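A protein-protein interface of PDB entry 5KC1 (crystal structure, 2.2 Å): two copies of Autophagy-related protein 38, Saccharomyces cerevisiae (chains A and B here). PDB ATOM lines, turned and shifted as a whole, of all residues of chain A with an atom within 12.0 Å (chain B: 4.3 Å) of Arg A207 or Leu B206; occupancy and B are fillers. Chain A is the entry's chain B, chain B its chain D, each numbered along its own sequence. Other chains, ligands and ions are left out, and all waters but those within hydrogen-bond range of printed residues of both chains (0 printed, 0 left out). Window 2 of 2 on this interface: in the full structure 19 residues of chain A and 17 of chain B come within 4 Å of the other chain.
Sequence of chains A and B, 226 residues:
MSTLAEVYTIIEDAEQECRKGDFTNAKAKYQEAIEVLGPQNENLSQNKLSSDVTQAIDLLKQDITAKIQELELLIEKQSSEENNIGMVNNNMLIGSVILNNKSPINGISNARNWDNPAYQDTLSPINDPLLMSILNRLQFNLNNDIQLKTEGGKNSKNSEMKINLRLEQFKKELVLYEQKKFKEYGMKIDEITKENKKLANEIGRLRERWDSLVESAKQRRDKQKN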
ATOM      1  N   LYS A 198      22.230 -26.942  22.005  1.00  0.00           N
ATOM      2  CA  LYS A 198      22.526 -25.620  22.548  1.00  0.00           C
ATOM      3  C   LYS A 198      23.516 -24.868  21.663  1.00  0.00           C
ATOM      4  O   LYS A 198      23.324 -23.689  21.368  1.00  0.00           O
ATOM      5  CB  LYS A 198      23.072 -25.734  23.973  1.00  0.00           C
ATOM      6  CG  LYS A 198      22.062 -26.244  24.993  1.00  0.00           C
ATOM      7  CD  LYS A 198      22.637 -26.215  26.402  1.00  0.00           C
ATOM      8  CE  LYS A 198      21.615 -26.670  27.436  1.00  0.00           C
ATOM      9  NZ  LYS A 198      22.162 -26.608  28.823  1.00  0.00           N
ATOM     10  N   LEU A 199      24.572 -25.557  21.243  1.00  0.00           N
ATOM     11  CA  LEU A 199      25.560 -24.962  20.353  1.00  0.00           C
ATOM     12  C   LEU A 199      24.947 -24.645  18.992  1.00  0.00           C
ATOM     13  O   LEU A 199      25.291 -23.645  18.365  1.00  0.00           O
ATOM     14  CB  LEU A 199      26.764 -25.890  20.185  1.00  0.00           C
ATOM     15  CG  LEU A 199      27.550 -26.203  21.458  1.00  0.00           C
ATOM     16  CD1 LEU A 199      28.823 -26.965  21.127  1.00  0.00           C
ATOM     17  CD2 LEU A 199      27.862 -24.928  22.222  1.00  0.00           C
ATOM     18  N   ALA A 200      24.035 -25.502  18.542  1.00  0.00           N
ATOM     19  CA  ALA A 200      23.355 -25.292  17.269  1.00  0.00           C
ATOM     20  C   ALA A 200      22.338 -24.158  17.374  1.00  0.00           C
ATOM     21  O   ALA A 200      21.942 -23.575  16.365  1.00  0.00           O
ATOM     22  CB  ALA A 200      22.678 -26.575  16.811  1.00  0.00           C
ATOM     23  N   ASN A 201      21.917 -23.851  18.597  1.00  0.00           N
ATOM     24  CA  ASN A 201      20.993 -22.746  18.835  1.00  0.00           C
ATOM     25  C   ASN A 201      21.734 -21.451  19.154  1.00  0.00           C
ATOM     26  O   ASN A 201      21.128 -20.450  19.538  1.00  0.00           O
ATOM     27  CB  ASN A 201      20.023 -23.090  19.968  1.00  0.00           C
ATOM     28  CG  ASN A 201      19.059 -24.200  19.594  1.00  0.00           C
ATOM     29  OD1 ASN A 201      18.826 -24.465  18.414  1.00  0.00           O
ATOM     30  ND2 ASN A 201      18.492 -24.856  20.600  1.00  0.00           N
ATOM     31  N   GLU A 202      23.053 -21.484  18.996  1.00  0.00           N
ATOM     32  CA  GLU A 202      23.880 -20.295  19.163  1.00  0.00           C
ATOM     33  C   GLU A 202      24.575 -19.951  17.851  1.00  0.00           C
ATOM     34  O   GLU A 202      24.648 -18.784  17.465  1.00  0.00           O
ATOM     35  CB  GLU A 202      24.916 -20.499  20.270  1.00  0.00           C
ATOM     36  CG  GLU A 202      24.323 -20.645  21.661  1.00  0.00           C
ATOM     37  CD  GLU A 202      25.387 -20.721  22.740  1.00  0.00           C
ATOM     38  OE1 GLU A 202      26.587 -20.651  22.399  1.00  0.00           O
ATOM     39  OE2 GLU A 202      25.023 -20.847  23.929  1.00  0.00           O
ATOM     40  N   ILE A 203      25.082 -20.975  17.170  1.00  0.00           N
ATOM     41  CA  ILE A 203      25.739 -20.790  15.882  1.00  0.00           C
ATOM     42  C   ILE A 203      24.763 -20.285  14.825  1.00  0.00           C
ATOM     43  O   ILE A 203      25.040 -19.308  14.131  1.00  0.00           O
ATOM     44  CB  ILE A 203      26.383 -22.095  15.381  1.00  0.00           C
ATOM     45  CG1 ILE A 203      27.592 -22.454  16.243  1.00  0.00           C
ATOM     46  CG2 ILE A 203      26.795 -21.959  13.924  1.00  0.00           C
ATOM     47  CD1 ILE A 203      28.342 -23.678  15.764  1.00  0.00           C
ATOM     48  N   GLY A 204      23.621 -20.955  14.710  1.00  0.00           N
ATOM     49  CA  GLY A 204      22.613 -20.582  13.735  1.00  0.00           C
ATOM     50  C   GLY A 204      22.015 -19.212  14.000  1.00  0.00           C
ATOM     51  O   GLY A 204      21.380 -18.623  13.124  1.00  0.00           O
ATOM     52  N   ARG A 205      22.220 -18.706  15.211  1.00  0.00           N
ATOM     53  CA  ARG A 205      21.695 -17.402  15.595  1.00  0.00           C
ATOM     54  C   ARG A 205      22.685 -16.287  15.271  1.00  0.00           C
ATOM     55  O   ARG A 205      22.288 -15.155  14.995  1.00  0.00           O
ATOM     56  CB  ARG A 205      21.350 -17.381  17.086  1.00  0.00           C
ATOM     57  CG  ARG A 205      20.753 -16.067  17.567  1.00  0.00           C
ATOM     58  CD  ARG A 205      20.447 -16.107  19.055  1.00  0.00           C
ATOM     59  NE  ARG A 205      21.640 -16.375  19.853  1.00  0.00           N
ATOM     60  CZ  ARG A 205      22.468 -15.436  20.298  1.00  0.00           C
ATOM     61  NH1 ARG A 205      22.236 -14.159  20.023  1.00  0.00           N
ATOM     62  NH2 ARG A 205      23.530 -15.772  21.018  1.00  0.00           N
ATOM     63  N   LEU A 206      23.974 -16.613  15.305  1.00  0.00           N
ATOM     64  CA  LEU A 206      25.017 -15.627  15.047  1.00  0.00           C
ATOM     65  C   LEU A 206      25.174 -15.353  13.555  1.00  0.00           C
ATOM     66  O   LEU A 206      25.223 -14.198  13.133  1.00  0.00           O
ATOM     67  CB  LEU A 206      26.349 -16.088  15.637  1.00  0.00           C
ATOM     68  CG  LEU A 206      26.366 -16.299  17.152  1.00  0.00           C
ATOM     69  CD1 LEU A 206      27.796 -16.400  17.666  1.00  0.00           C
ATOM     70  CD2 LEU A 206      25.608 -15.188  17.865  1.00  0.00           C
ATOM     71  N   ARG A 207      25.253 -16.420  12.766  1.00  0.00           N
ATOM     72  CA  ARG A 207      25.392 -16.297  11.319  1.00  0.00           C
ATOM     73  C   ARG A 207      24.209 -15.533  10.734  1.00  0.00           C
ATOM     74  O   ARG A 207      24.386 -14.612   9.939  1.00  0.00           O
ATOM     75  CB  ARG A 207      25.509 -17.678  10.672  1.00  0.00           C
ATOM     76  CG  ARG A 207      26.308 -18.669  11.501  1.00  0.00           C
ATOM     77  CD  ARG A 207      26.567 -19.963  10.752  1.00  0.00           C
ATOM     78  NE  ARG A 207      27.918 -20.004  10.199  1.00  0.00           N
ATOM     79  CZ  ARG A 207      28.441 -21.057   9.581  1.00  0.00           C
ATOM     80  NH1 ARG A 207      27.726 -22.165   9.432  1.00  0.00           N
ATOM     81  NH2 ARG A 207      29.680 -21.004   9.112  1.00  0.00           N
ATOM     82  N   GLU A 208      23.004 -15.918  11.147  1.00  0.00           N
ATOM     83  CA  GLU A 208      21.784 -15.234  10.729  1.00  0.00           C
ATOM     84  C   GLU A 208      21.856 -13.753  11.092  1.00  0.00           C
ATOM     85  O   GLU A 208      21.527 -12.882  10.285  1.00  0.00           O
ATOM     86  CB  GLU A 208      20.559 -15.883  11.376  1.00  0.00           C
ATOM     87  CG  GLU A 208      19.229 -15.391  10.830  1.00  0.00           C
ATOM     88  CD  GLU A 208      19.018 -15.774   9.378  1.00  0.00           C
ATOM     89  OE1 GLU A 208      19.742 -16.664   8.884  1.00  0.00           O
ATOM     90  OE2 GLU A 208      18.128 -15.184   8.730  1.00  0.00           O
ATOM     91  N   ARG A 209      22.294 -13.483  12.318  1.00  0.00           N
ATOM     92  CA  ARG A 209      22.547 -12.124  12.783  1.00  0.00           C
ATOM     93  C   ARG A 209      23.685 -11.487  11.991  1.00  0.00           C
ATOM     94  O   ARG A 209      23.598 -10.333  11.569  1.00  0.00           O
ATOM     95  CB  ARG A 209      22.883 -12.139  14.274  1.00  0.00           C
ATOM     96  CG  ARG A 209      23.511 -10.866  14.800  1.00  0.00           C
ATOM     97  CD  ARG A 209      24.343 -11.170  16.032  1.00  0.00           C
ATOM     98  NE  ARG A 209      24.552  -9.997  16.872  1.00  0.00           N
ATOM     99  CZ  ARG A 209      25.241 -10.009  18.008  1.00  0.00           C
ATOM    100  NH1 ARG A 209      25.380  -8.896  18.715  1.00  0.00           N
ATOM    101  NH2 ARG A 209      25.791 -11.137  18.437  1.00  0.00           N
ATOM    102  N   TRP A 210      24.752 -12.257  11.800  1.00  0.00           N
ATOM    103  CA  TRP A 210      25.912 -11.828  11.029  1.00  0.00           C
ATOM    104  C   TRP A 210      25.531 -11.446   9.602  1.00  0.00           C
ATOM    105  O   TRP A 210      25.977 -10.422   9.084  1.00  0.00           O
ATOM    106  CB  TRP A 210      26.966 -12.940  11.022  1.00  0.00           C
ATOM    107  CG  TRP A 210      28.082 -12.748  10.041  1.00  0.00           C
ATOM    108  CD1 TRP A 210      28.078 -13.091   8.719  1.00  0.00           C
ATOM    109  CD2 TRP A 210      29.373 -12.192  10.307  1.00  0.00           C
ATOM    110  NE1 TRP A 210      29.283 -12.772   8.144  1.00  0.00           N
ATOM    111  CE2 TRP A 210      30.100 -12.217   9.101  1.00  0.00           C
ATOM    112  CE3 TRP A 210      29.990 -11.667  11.448  1.00  0.00           C
ATOM    113  CZ2 TRP A 210      31.404 -11.742   8.997  1.00  0.00           C
ATOM    114  CZ3 TRP A 210      31.286 -11.195  11.348  1.00  0.00           C
ATOM    115  CH2 TRP A 210      31.979 -11.235  10.131  1.00  0.00           C
ATOM    116  N   ASP A 211      24.704 -12.275   8.972  1.00  0.00           N
ATOM    117  CA  ASP A 211      24.255 -12.033   7.603  1.00  0.00           C
ATOM    118  C   ASP A 211      23.499 -10.712   7.475  1.00  0.00           C
ATOM    119  O   ASP A 211      23.120 -10.098   8.473  1.00  0.00           O
ATOM    120  CB  ASP A 211      23.371 -13.186   7.118  1.00  0.00           C
ATOM    121  CG  ASP A 211      24.174 -14.334   6.531  1.00  0.00           C
ATOM    122  OD1 ASP A 211      24.634 -15.203   7.300  1.00  0.00           O
ATOM    123  OD2 ASP A 211      24.337 -14.371   5.294  1.00  0.00           O
ATOM    124  N   GLU B 202      33.461 -23.384  15.433  1.00  0.00           N
ATOM    125  CA  GLU B 202      32.750 -22.375  14.658  1.00  0.00           C
ATOM    126  C   GLU B 202      32.267 -21.238  15.552  1.00  0.00           C
ATOM    127  O   GLU B 202      32.154 -20.095  15.111  1.00  0.00           O
ATOM    128  CB  GLU B 202      31.569 -22.998  13.913  1.00  0.00           C
ATOM    129  CG  GLU B 202      31.970 -24.015  12.858  1.00  0.00           C
ATOM    130  CD  GLU B 202      30.803 -24.442  11.989  1.00  0.00           C
ATOM    131  OE1 GLU B 202      29.718 -23.834  12.108  1.00  0.00           O
ATOM    132  OE2 GLU B 202      30.971 -25.386  11.188  1.00  0.00           O
ATOM    133  N   ILE B 203      31.980 -21.559  16.809  1.00  0.00           N
ATOM    134  CA  ILE B 203      31.590 -20.547  17.782  1.00  0.00           C
ATOM    135  C   ILE B 203      32.806 -19.754  18.242  1.00  0.00           C
ATOM    136  O   ILE B 203      32.729 -18.544  18.455  1.00  0.00           O
ATOM    137  CB  ILE B 203      30.897 -21.168  19.008  1.00  0.00           C
ATOM    138  CG1 ILE B 203      29.550 -21.772  18.610  1.00  0.00           C
ATOM    139  CG2 ILE B 203      30.701 -20.124  20.093  1.00  0.00           C
ATOM    140  CD1 ILE B 203      28.755 -22.314  19.775  1.00  0.00           C
ATOM    141  N   GLY B 204      33.930 -20.448  18.390  1.00  0.00           N
ATOM    142  CA  GLY B 204      35.168 -19.816  18.807  1.00  0.00           C
ATOM    143  C   GLY B 204      35.677 -18.835  17.770  1.00  0.00           C
ATOM    144  O   GLY B 204      36.393 -17.888  18.094  1.00  0.00           O
ATOM    145  N   ARG B 205      35.302 -19.065  16.516  1.00  0.00           N
ATOM    146  CA  ARG B 205      35.698 -18.180  15.429  1.00  0.00           C
ATOM    147  C   ARG B 205      34.755 -16.986  15.319  1.00  0.00           C
ATOM    148  O   ARG B 205      35.198 -15.839  15.331  1.00  0.00           O
ATOM    149  CB  ARG B 205      35.748 -18.945  14.104  1.00  0.00           C
ATOM    150  CG  ARG B 205      36.903 -19.929  14.016  1.00  0.00           C
ATOM    151  CD  ARG B 205      36.947 -20.633  12.671  1.00  0.00           C
ATOM    152  NE  ARG B 205      38.155 -21.441  12.524  1.00  0.00           N
ATOM    153  CZ  ARG B 205      38.265 -22.705  12.921  1.00  0.00           C
ATOM    154  NH1 ARG B 205      37.236 -23.315  13.494  1.00  0.00           N
ATOM    155  NH2 ARG B 205      39.405 -23.360  12.747  1.00  0.00           N
ATOM    156  N   LEU B 206      33.456 -17.259  15.234  1.00  0.00           N
ATOM    157  CA  LEU B 206      32.453 -16.206  15.078  1.00  0.00           C
ATOM    158  C   LEU B 206      32.447 -15.214  16.242  1.00  0.00           C
ATOM    159  O   LEU B 206      31.802 -14.169  16.168  1.00  0.00           O
ATOM    160  CB  LEU B 206      31.059 -16.817  14.916  1.00  0.00           C
ATOM    161  CG  LEU B 206      30.852 -17.717  13.696  1.00  0.00           C
ATOM    162  CD1 LEU B 206      29.369 -17.947  13.443  1.00  0.00           C
ATOM    163  CD2 LEU B 206      31.529 -17.127  12.468  1.00  0.00           C
ATOM    164  N   ARG B 207      33.158 -15.547  17.315  1.00  0.00           N
ATOM    165  CA  ARG B 207      33.334 -14.619  18.426  1.00  0.00           C
ATOM    166  C   ARG B 207      34.647 -13.857  18.289  1.00  0.00           C
ATOM    167  O   ARG B 207      34.729 -12.674  18.621  1.00  0.00           O
ATOM    168  CB  ARG B 207      33.300 -15.351  19.768  1.00  0.00           C
ATOM    169  CG  ARG B 207      31.911 -15.740  20.243  1.00  0.00           C
ATOM    170  CD  ARG B 207      31.882 -15.863  21.760  1.00  0.00           C
ATOM    171  NE  ARG B 207      30.598 -16.349  22.255  1.00  0.00           N
ATOM    172  CZ  ARG B 207      30.376 -17.599  22.649  1.00  0.00           C
ATOM    173  NH1 ARG B 207      31.356 -18.491  22.611  1.00  0.00           N
ATOM    174  NH2 ARG B 207      29.176 -17.956  23.086  1.00  0.00           N
ATOM    175  N   GLU B 208      35.675 -14.544  17.799  1.00  0.00           N
ATOM    176  CA  GLU B 208      36.991 -13.938  17.640  1.00  0.00           C
ATOM    177  C   GLU B 208      37.027 -13.034  16.410  1.00  0.00           C
ATOM    178  O   GLU B 208      37.913 -12.191  16.278  1.00  0.00           O
ATOM    179  CB  GLU B 208      38.072 -15.017  17.542  1.00  0.00           C
ATOM    180  CG  GLU B 208      39.493 -14.508  17.750  1.00  0.00           C
ATOM    181  CD  GLU B 208      39.764 -14.067  19.180  1.00  0.00           C
ATOM    182  OE1 GLU B 208      38.803 -13.968  19.972  1.00  0.00           O
ATOM    183  OE2 GLU B 208      40.944 -13.823  19.513  1.00  0.00           O
ATOM    184  N   ARG B 209      36.063 -13.217  15.514  1.00  0.00           N
ATOM    185  CA  ARG B 209      35.923 -12.340  14.356  1.00  0.00           C
ATOM    186  C   ARG B 209      35.590 -10.926  14.818  1.00  0.00           C
ATOM    187  O   ARG B 209      36.265  -9.964  14.449  1.00  0.00           O
ATOM    188  CB  ARG B 209      34.837 -12.850  13.406  1.00  0.00           C
ATOM    189  CG  ARG B 209      35.024 -14.285  12.943  1.00  0.00           C
ATOM    190  CD  ARG B 209      36.356 -14.485  12.244  1.00  0.00           C
ATOM    191  NE  ARG B 209      36.522 -13.566  11.122  1.00  0.00           N
ATOM    192  CZ  ARG B 209      35.750 -13.561  10.040  1.00  0.00           C
ATOM    193  NH1 ARG B 209      34.747 -14.423   9.933  1.00  0.00           N
ATOM    194  NH2 ARG B 209      35.975 -12.689   9.068  1.00  0.00           N
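The side-chain carboxylate (OE1) of Glu B202 is in salt-bridge range of the guanidinium group (NH1) of Arg A207, at 3.7 Å. The guanidinium group (NH2) of Arg B207 lies within salt-bridge range of the side-chain carboxylate (OE1) of Glu A202, 3.8 Å away.
Leu A199 touches Ile B203. Glu A202 touches Ile B203. Ile A203 touches Glu B202. CG1 of Ile B203 touches CG1 of Ile A203, 3.1 Å away. Arg A207 touches Leu B206 (CG to CD1, 3.7 Å).
Of the 14 printed residues of chain A, 4 touch a printed residue of chain B. Hydrophobic or aromatic side chains of chain A that line the printed part of chain B: Leu A199 and Ile A203. Along chain A the printed residues that touch a printed residue of chain B span positions 199 to 207. Among the printed residues, 7 pairs touch across the chains.
Glu A202 touches Ile B203, and with the chains exchanged Ile A203 touches Glu B202. Glu A202 touches Arg B207, and with the chains exchanged Arg A207 touches Glu B202. Ile A203 touches its own counterpart, Ile B203. Arg A207 touches Leu B206, but with the chains exchanged Leu A206 does not touch Arg B207 (4.9 Å).
The side-chain carboxylate (OD1) of Asp A211 lies close to the backbone carbonyl oxygen (O) of Arg A207 (2.7 Å).
Of the printed residues of chain B, Leu A199 touches Ile B203 (3.7 Å). Printed residues of chain B within 4 Å of Glu A202: Ile B203 (3.8 Å) and Arg B207 (3.8 Å). Printed residues of chain B within 4 Å of Ile A203: Glu B202 and Ile B203. Arg A207 touches just these residues of chain B: Glu B202 (3.7 Å) and Leu B206 (3.7 Å). Of chain A, only Ile A203 (3.8 Å) and Arg A207 (3.7 Å) come within 4 Å of Glu B202. Gly B204 touches none of the printed residues of chain A. Of chain A, only Arg A207 comes within 4 Å of Leu B206. Printed residues of chain A within 4 Å of Arg B207: Glu A202. No residue of chain A comes within 4 Å of Arg B209. The nearest printed residue of chain B that does not touch Arg A207 is Ile B203 (7.9 Å). The nearest residue of chain A that does not touch Leu B206 is Leu A206 (4.2 Å). The nearest printed residue of chain A that does not touch Arg B207 is Leu A206 (4.9 Å).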
